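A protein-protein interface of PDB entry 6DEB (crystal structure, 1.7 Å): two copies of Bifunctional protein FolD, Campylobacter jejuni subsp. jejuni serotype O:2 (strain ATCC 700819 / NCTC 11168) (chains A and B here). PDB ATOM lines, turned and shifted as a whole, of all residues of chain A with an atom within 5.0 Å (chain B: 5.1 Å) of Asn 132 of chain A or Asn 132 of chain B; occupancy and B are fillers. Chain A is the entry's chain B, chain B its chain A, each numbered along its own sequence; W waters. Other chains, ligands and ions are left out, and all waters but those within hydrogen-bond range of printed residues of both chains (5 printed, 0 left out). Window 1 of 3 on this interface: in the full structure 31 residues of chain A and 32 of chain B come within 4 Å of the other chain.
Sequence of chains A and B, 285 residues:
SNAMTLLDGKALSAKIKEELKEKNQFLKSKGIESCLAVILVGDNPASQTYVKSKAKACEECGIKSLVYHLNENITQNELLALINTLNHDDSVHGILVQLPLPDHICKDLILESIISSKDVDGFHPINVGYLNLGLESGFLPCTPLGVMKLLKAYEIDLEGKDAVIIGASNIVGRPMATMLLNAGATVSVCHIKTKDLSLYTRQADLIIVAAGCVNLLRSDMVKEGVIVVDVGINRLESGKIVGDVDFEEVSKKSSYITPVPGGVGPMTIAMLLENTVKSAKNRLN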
ATOM      1  N   VAL A 128     -24.910  22.440  13.364  1.00  0.00           N
ATOM      2  CA  VAL A 128     -24.623  21.504  14.445  1.00  0.00           C
ATOM      3  C   VAL A 128     -24.333  22.305  15.723  1.00  0.00           C
ATOM      4  O   VAL A 128     -24.807  21.977  16.819  1.00  0.00           O
ATOM      5  CB  VAL A 128     -23.435  20.605  14.075  1.00  0.00           C
ATOM      6  CG1 VAL A 128     -23.025  19.730  15.235  1.00  0.00           C
ATOM      7  CG2 VAL A 128     -23.768  19.732  12.831  1.00  0.00           C
ATOM      8  N   GLY A 129     -23.562  23.376  15.573  1.00  0.00           N
ATOM      9  CA  GLY A 129     -23.210  24.210  16.714  1.00  0.00           C
ATOM     10  C   GLY A 129     -24.428  24.881  17.351  1.00  0.00           C
ATOM     11  O   GLY A 129     -24.570  24.879  18.566  1.00  0.00           O
ATOM     12  N   TYR A 130     -25.304  25.454  16.533  1.00  0.00           N
ATOM     13  CA  TYR A 130     -26.490  26.136  17.064  1.00  0.00           C
ATOM     14  C   TYR A 130     -27.317  25.167  17.904  1.00  0.00           C
ATOM     15  O   TYR A 130     -27.746  25.501  18.985  1.00  0.00           O
ATOM     16  CB  TYR A 130     -27.375  26.652  15.927  1.00  0.00           C
ATOM     17  CG  TYR A 130     -26.851  27.871  15.195  1.00  0.00           C
ATOM     18  CD1 TYR A 130     -26.147  28.864  15.854  1.00  0.00           C
ATOM     19  CD2 TYR A 130     -27.060  28.012  13.822  1.00  0.00           C
ATOM     20  CE1 TYR A 130     -25.665  29.993  15.154  1.00  0.00           C
ATOM     21  CE2 TYR A 130     -26.602  29.121  13.125  1.00  0.00           C
ATOM     22  CZ  TYR A 130     -25.901  30.110  13.786  1.00  0.00           C
ATOM     23  OH  TYR A 130     -25.456  31.218  13.079  1.00  0.00           O
ATOM     24  N   LEU A 131     -27.504  23.958  17.395  1.00  0.00           N
ATOM     25  CA  LEU A 131     -28.298  22.962  18.122  1.00  0.00           C
ATOM     26  C   LEU A 131     -27.643  22.576  19.432  1.00  0.00           C
ATOM     27  O   LEU A 131     -28.312  22.456  20.454  1.00  0.00           O
ATOM     28  CB  LEU A 131     -28.526  21.728  17.251  1.00  0.00           C
ATOM     29  CG  LEU A 131     -29.121  20.518  17.978  1.00  0.00           C
ATOM     30  CD1 LEU A 131     -30.511  20.865  18.510  1.00  0.00           C
ATOM     31  CD2 LEU A 131     -29.195  19.337  16.994  1.00  0.00           C
ATOM     32  N   ASN A 132     -26.318  22.378  19.406  1.00  0.00           N
ATOM     33  CA  ASN A 132     -25.614  22.011  20.637  1.00  0.00           C
ATOM     34  C   ASN A 132     -25.598  23.149  21.659  1.00  0.00           C
ATOM     35  O   ASN A 132     -25.472  22.913  22.862  1.00  0.00           O
ATOM     36  CB  ASN A 132     -24.184  21.567  20.296  1.00  0.00           C
ATOM     37  CG  ASN A 132     -23.533  20.803  21.428  1.00  0.00           C
ATOM     38  OD1 ASN A 132     -22.776  21.361  22.228  1.00  0.00           O
ATOM     39  ND2 ASN A 132     -23.856  19.515  21.523  1.00  0.00           N
ATOM     40  N   LEU A 133     -25.722  24.387  21.189  1.00  0.00           N
ATOM     41  CA  LEU A 133     -25.837  25.535  22.101  1.00  0.00           C
ATOM     42  C   LEU A 133     -27.231  25.688  22.675  1.00  0.00           C
ATOM     43  O   LEU A 133     -27.463  26.553  23.522  1.00  0.00           O
ATOM     44  CB  LEU A 133     -25.442  26.831  21.389  1.00  0.00           C
ATOM     45  CG  LEU A 133     -23.955  26.899  21.050  1.00  0.00           C
ATOM     46  CD1 LEU A 133     -23.661  28.057  20.113  1.00  0.00           C
ATOM     47  CD2 LEU A 133     -23.129  27.038  22.345  1.00  0.00           C
ATOM     48  N   GLY A 134     -28.150  24.832  22.237  1.00  0.00           N
ATOM     49  CA  GLY A 134     -29.509  24.815  22.764  1.00  0.00           C
ATOM     50  C   GLY A 134     -30.466  25.683  21.967  1.00  0.00           C
ATOM     51  O   GLY A 134     -31.634  25.875  22.345  1.00  0.00           O
ATOM     52  N   ASN A 170     -23.227  11.245  13.463  1.00  0.00           N
ATOM     53  CA  ASN A 170     -23.581  12.654  13.239  1.00  0.00           C
ATOM     54  C   ASN A 170     -24.955  12.804  12.624  1.00  0.00           C
ATOM     55  O   ASN A 170     -25.636  13.819  12.817  1.00  0.00           O
ATOM     56  CB  ASN A 170     -22.566  13.323  12.329  1.00  0.00           C
ATOM     57  CG  ASN A 170     -21.204  13.458  12.996  1.00  0.00           C
ATOM     58  OD1 ASN A 170     -21.118  13.537  14.217  1.00  0.00           O
ATOM     59  ND2 ASN A 170     -20.136  13.502  12.189  1.00  0.00           N
ATOM     60  N   ARG A 174     -25.918  11.633  17.678  1.00  0.00           N
ATOM     61  CA  ARG A 174     -25.458  12.826  18.395  1.00  0.00           C
ATOM     62  C   ARG A 174     -26.527  13.936  18.452  1.00  0.00           C
ATOM     63  O   ARG A 174     -26.860  14.401  19.549  1.00  0.00           O
ATOM     64  CB  ARG A 174     -24.128  13.353  17.831  1.00  0.00           C
ATOM     65  CG  ARG A 174     -22.983  12.394  18.160  1.00  0.00           C
ATOM     66  CD  ARG A 174     -21.745  12.735  17.401  1.00  0.00           C
ATOM     67  NE  ARG A 174     -20.684  11.784  17.732  1.00  0.00           N
ATOM     68  CZ  ARG A 174     -19.510  12.141  18.245  1.00  0.00           C
ATOM     69  NH1 ARG A 174     -19.226  13.426  18.452  1.00  0.00           N
ATOM     70  NH2 ARG A 174     -18.596  11.209  18.509  1.00  0.00           N
ATOM     71  N   THR A 178     -28.674  15.432  21.725  1.00  0.00           N
ATOM     72  CA  THR A 178     -28.699  16.857  22.008  1.00  0.00           C
ATOM     73  C   THR A 178     -30.121  17.369  22.065  1.00  0.00           C
ATOM     74  O   THR A 178     -30.454  18.172  22.939  1.00  0.00           O
ATOM     75  CB  THR A 178     -27.881  17.638  20.980  1.00  0.00           C
ATOM     76  OG1 THR A 178     -26.532  17.165  21.038  1.00  0.00           O
ATOM     77  CG2 THR A 178     -27.888  19.151  21.284  1.00  0.00           C
ATOM     78  N   VAL B 128     -18.112  24.973  18.074  1.00  0.00           N
ATOM     79  CA  VAL B 128     -18.933  23.995  18.772  1.00  0.00           C
ATOM     80  C   VAL B 128     -19.320  22.883  17.792  1.00  0.00           C
ATOM     81  O   VAL B 128     -19.274  21.689  18.140  1.00  0.00           O
ATOM     82  CB  VAL B 128     -20.196  24.686  19.348  1.00  0.00           C
ATOM     83  CG1 VAL B 128     -21.122  23.658  19.966  1.00  0.00           C
ATOM     84  CG2 VAL B 128     -19.779  25.773  20.364  1.00  0.00           C
ATOM     85  N   GLY B 129     -19.688  23.278  16.572  1.00  0.00           N
ATOM     86  CA  GLY B 129     -20.067  22.315  15.541  1.00  0.00           C
ATOM     87  C   GLY B 129     -18.935  21.371  15.190  1.00  0.00           C
ATOM     88  O   GLY B 129     -19.121  20.160  15.106  1.00  0.00           O
ATOM     89  N   TYR B 130     -17.746  21.923  14.966  1.00  0.00           N
ATOM     90  CA  TYR B 130     -16.615  21.074  14.570  1.00  0.00           C
ATOM     91  C   TYR B 130     -16.358  20.012  15.634  1.00  0.00           C
ATOM     92  O   TYR B 130     -16.159  18.836  15.313  1.00  0.00           O
ATOM     93  CB  TYR B 130     -15.345  21.912  14.384  1.00  0.00           C
ATOM     94  CG  TYR B 130     -15.314  22.794  13.157  1.00  0.00           C
ATOM     95  CD1 TYR B 130     -15.774  22.341  11.926  1.00  0.00           C
ATOM     96  CD2 TYR B 130     -14.751  24.068  13.218  1.00  0.00           C
ATOM     97  CE1 TYR B 130     -15.705  23.146  10.796  1.00  0.00           C
ATOM     98  CE2 TYR B 130     -14.672  24.874  12.100  1.00  0.00           C
ATOM     99  CZ  TYR B 130     -15.159  24.420  10.892  1.00  0.00           C
ATOM    100  OH  TYR B 130     -15.078  25.236   9.776  1.00  0.00           O
ATOM    101  N   LEU B 131     -16.352  20.420  16.901  1.00  0.00           N
ATOM    102  CA  LEU B 131     -16.147  19.454  17.987  1.00  0.00           C
ATOM    103  C   LEU B 131     -17.220  18.360  17.997  1.00  0.00           C
ATOM    104  O   LEU B 131     -16.920  17.176  18.170  1.00  0.00           O
ATOM    105  CB  LEU B 131     -16.058  20.168  19.342  1.00  0.00           C
ATOM    106  CG  LEU B 131     -16.084  19.303  20.608  1.00  0.00           C
ATOM    107  CD1 LEU B 131     -14.876  18.357  20.590  1.00  0.00           C
ATOM    108  CD2 LEU B 131     -16.067  20.193  21.881  1.00  0.00           C
ATOM    109  N   ASN B 132     -18.478  18.771  17.833  1.00  0.00           N
ATOM    110  CA  ASN B 132     -19.574  17.815  17.871  1.00  0.00           C
ATOM    111  C   ASN B 132     -19.557  16.848  16.704  1.00  0.00           C
ATOM    112  O   ASN B 132     -20.040  15.713  16.822  1.00  0.00           O
ATOM    113  CB  ASN B 132     -20.917  18.527  17.947  1.00  0.00           C
ATOM    114  CG  ASN B 132     -21.989  17.635  18.506  1.00  0.00           C
ATOM    115  OD1 ASN B 132     -22.830  17.119  17.757  1.00  0.00           O
ATOM    116  ND2 ASN B 132     -21.993  17.456  19.816  1.00  0.00           N
ATOM    117  N   LEU B 133     -18.980  17.277  15.577  1.00  0.00           N
ATOM    118  CA  LEU B 133     -18.813  16.380  14.438  1.00  0.00           C
ATOM    119  C   LEU B 133     -17.610  15.462  14.592  1.00  0.00           C
ATOM    120  O   LEU B 133     -17.355  14.620  13.719  1.00  0.00           O
ATOM    121  CB  LEU B 133     -18.664  17.196  13.146  1.00  0.00           C
ATOM    122  CG  LEU B 133     -19.913  17.958  12.731  1.00  0.00           C
ATOM    123  CD1 LEU B 133     -19.566  18.946  11.622  1.00  0.00           C
ATOM    124  CD2 LEU B 133     -21.027  17.028  12.270  1.00  0.00           C
ATOM    125  N   GLY B 134     -16.852  15.647  15.669  1.00  0.00           N
ATOM    126  CA  GLY B 134     -15.646  14.870  15.887  1.00  0.00           C
ATOM    127  C   GLY B 134     -14.517  15.292  14.956  1.00  0.00           C
ATOM    128  O   GLY B 134     -13.642  14.482  14.625  1.00  0.00           O
ATOM    129  N   ASN B 170     -22.808  25.120  28.402  1.00  0.00           N
ATOM    130  CA  ASN B 170     -22.067  25.239  27.140  1.00  0.00           C
ATOM    131  C   ASN B 170     -20.577  25.424  27.399  1.00  0.00           C
ATOM    132  O   ASN B 170     -19.745  25.080  26.563  1.00  0.00           O
ATOM    133  CB  ASN B 170     -22.596  26.391  26.303  1.00  0.00           C
ATOM    134  CG  ASN B 170     -24.002  26.127  25.765  1.00  0.00           C
ATOM    135  OD1 ASN B 170     -24.347  24.991  25.460  1.00  0.00           O
ATOM    136  ND2 ASN B 170     -24.809  27.180  25.658  1.00  0.00           N
ATOM    137  N   ARG B 174     -21.468  20.189  28.203  1.00  0.00           N
ATOM    138  CA  ARG B 174     -21.745  19.686  26.848  1.00  0.00           C
ATOM    139  C   ARG B 174     -20.456  19.382  26.064  1.00  0.00           C
ATOM    140  O   ARG B 174     -20.299  18.267  25.565  1.00  0.00           O
ATOM    141  CB  ARG B 174     -22.656  20.648  26.102  1.00  0.00           C
ATOM    142  CG  ARG B 174     -24.079  20.601  26.670  1.00  0.00           C
ATOM    143  CD  ARG B 174     -24.911  21.724  26.134  1.00  0.00           C
ATOM    144  NE  ARG B 174     -26.268  21.704  26.701  1.00  0.00           N
ATOM    145  CZ  ARG B 174     -27.381  21.551  25.989  1.00  0.00           C
ATOM    146  NH1 ARG B 174     -27.322  21.427  24.663  1.00  0.00           N
ATOM    147  NH2 ARG B 174     -28.570  21.556  26.596  1.00  0.00           N
ATOM    148  N   PRO B 175     -19.518  20.345  25.987  1.00  0.00           N
ATOM    149  CA  PRO B 175     -18.285  19.952  25.272  1.00  0.00           C
ATOM    150  C   PRO B 175     -17.513  18.841  25.977  1.00  0.00           C
ATOM    151  O   PRO B 175     -16.815  18.065  25.316  1.00  0.00           O
ATOM    152  CB  PRO B 175     -17.451  21.248  25.252  1.00  0.00           C
ATOM    153  CG  PRO B 175     -18.093  22.135  26.345  1.00  0.00           C
ATOM    154  CD  PRO B 175     -19.546  21.789  26.285  1.00  0.00           C
ATOM    155  N   THR B 178     -18.966  15.608  24.871  1.00  0.00           N
ATOM    156  CA  THR B 178     -18.619  15.383  23.474  1.00  0.00           C
ATOM    157  C   THR B 178     -17.154  14.917  23.337  1.00  0.00           C
ATOM    158  O   THR B 178     -16.848  14.003  22.558  1.00  0.00           O
ATOM    159  CB  THR B 178     -18.895  16.655  22.652  1.00  0.00           C
ATOM    160  OG1 THR B 178     -20.298  16.908  22.705  1.00  0.00           O
ATOM    161  CG2 THR B 178     -18.461  16.480  21.207  1.00  0.00           C
ATOM    162  N   ASN B 182     -16.023  11.352  21.873  1.00  0.00           N
ATOM    163  CA  ASN B 182     -15.034  11.317  20.794  1.00  0.00           C
ATOM    164  C   ASN B 182     -13.906  10.364  21.126  1.00  0.00           C
ATOM    165  O   ASN B 182     -13.344   9.718  20.224  1.00  0.00           O
ATOM    166  CB  ASN B 182     -14.481  12.725  20.486  1.00  0.00           C
ATOM    167  CG  ASN B 182     -15.496  13.617  19.777  1.00  0.00           C
ATOM    168  OD1 ASN B 182     -16.531  13.153  19.310  1.00  0.00           O
ATOM    169  ND2 ASN B 182     -15.176  14.902  19.656  1.00  0.00           N
HETATM  170  O   HOH W   1     -16.995  13.590  11.260  1.00  0.00           O
HETATM  171  O   HOH W   2     -22.879  15.619  15.238  1.00  0.00           O
HETATM  172  O   HOH W   3     -24.921  18.043  19.244  1.00  0.00           O
HETATM  173  O   HOH W   4     -22.469  23.594  23.925  1.00  0.00           O
HETATM  174  O   HOH W   5     -20.897  19.195  21.944  1.00  0.00           O
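Water W5 lies within hydrogen-bond range of the side-chain hydroxyl of Thr 178 of chain B, the side-chain amide oxygen of Asn 132 of chain A and the side-chain amide nitrogen of Asn 132 of chain B.
Water W3 lies within hydrogen-bond range of OG1 of Thr 178 of chain A (2.6 Å), OD1 of Asn 132 of chain B (2.7 Å) and ND2 of Asn 132 of chain A (2.9 Å).
Water W1 bridges O of Leu 133 of chain B and ND2 of Asn 170 of chain A.
Water W4 lies within hydrogen-bond range of the side-chain amide oxygen of Asn 170 of chain B (2.8 Å) and the side-chain amide oxygen of Asn 132 of chain A (2.8 Å).
Water W2 bridges OD1 of Asn 170 of chain A (2.9 Å) and OD1 of Asn 132 of chain B (2.9 Å).
Val 128 of chain A touches Gly 129 of chain B, and with the chains exchanged Gly 129 of chain A touches Val 128 of chain B.
Gly 129 of chain A touches its own counterpart, Gly 129 of chain B.
Asn 132 of chain A touches Asn 170 of chain B, and with the chains exchanged Asn 170 of chain A touches Asn 132 of chain B.
Leu 133 of chain A touches Asn 170 of chain B, and with the chains exchanged Asn 170 of chain A touches Leu 133 of chain B.
Printed residues of chain B that touch a printed residue of chain A: Val 128, Gly 129, Asn 132, Leu 133, Asn 170, Arg 174 and Asn 182.
Hydrophobic or aromatic side chains of chain B within 4 Å of the printed part of chain A: Val 128 and Leu 133.
Of the 10 printed residues of chain A, 6 touch a printed residue of chain B.
Hydrophobic or aromatic side chains of chain A that line the printed part of chain B: Val 128 and Leu 133.
ND2 of Asn 170 of chain A lies within hydrogen-bond range of O of Leu 133 of chain B.
ND2 of Asn 132 of chain B sits close to ND2 of Asn 132 of chain A, 3.3 Å away.
The backbone carbonyl oxygen of Leu 133 of chain A is in hydrogen-bond range of the side-chain amide nitrogen of Asn 170 of chain B (3.5 Å).
The guanidinium group (NH1) of Arg 174 of chain A lies within hydrogen-bond range of the backbone carbonyl oxygen (O) of Asn 132 of chain B (2.9 Å).
The side-chain amide oxygen (OD1) of Asn 182 of chain B sits at hydrogen-bond distance from the guanidinium group (NH1) of Arg 174 of chain A (2.8 Å).
NH1 of Arg 174 of chain B lies within hydrogen-bond range of O of Asn 132 of chain A (3.0 Å).
CG1 of Val 128 of chain A touches O of Gly 129 of chain B, at 3.9 Å.
OD1 of Asn 132 of chain B touches CG1 of Val 128 of chain A (3.6 Å).
Val 128 of chain A touches Leu 133 of chain B (CG2 to CD2, 3.9 Å).
Val 128 of chain B touches Gly 129 of chain A (CG1 to CA, 3.9 Å).
Gly 129 of chain A touches Gly 129 of chain B (CA to N, 3.6 Å).
Val 128 of chain B touches Asn 132 of chain A (CG1 to OD1, 3.6 Å).
Asn 132 of chain A touches Asn 170 of chain B (O to OD1, 3.5 Å).
Asn 170 of chain A touches Asn 132 of chain B (OD1 to O, 3.6 Å).
O of Leu 131 of chain B lies within hydrogen-bond range of ND2 of Asn 182 of chain B (3.2 Å).
The backbone carbonyl oxygen (O) of Arg 174 of chain B sits at hydrogen-bond distance from the side-chain hydroxyl (OG1) of Thr 178 of chain B, 3.2 Å away.
ND2 of Asn 132 of chain B lies within hydrogen-bond range of OG1 of Thr 178 of chain B, 3.4 Å away.
The side-chain hydroxyl (OG1) of Thr 178 of chain A sits at hydrogen-bond distance from the backbone carbonyl oxygen (O) of Arg 174 of chain A.
OD1 of Asn 182 of chain B lies close to O of Thr 178 of chain B.
Of chain B, only Val 128, Asn 132, Asn 170 and Arg 174 come within 4 Å of Asn 132 of chain A.
Of chain A, only Val 128, Asn 132, Asn 170 and Arg 174 come within 4 Å of Asn 132 of chain B.
Printed residues of chain A within 4 Å of Asn 170 of chain B: Asn 132 and Leu 133.
Printed residues of chain B within 4 Å of Asn 170 of chain A: Asn 132 (3.6 Å) and Leu 133 (3.4 Å).
Printed residues of chain A within 4 Å of Asn 182 of chain B: Arg 174 (2.8 Å).
The nearest residue of chain B that does not touch Asn 132 of chain A is Thr 178 of chain B (4.6 Å).
The nearest printed residue of chain A that does not touch Leu 133 of chain B is Arg 174 of chain A (4.7 Å).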
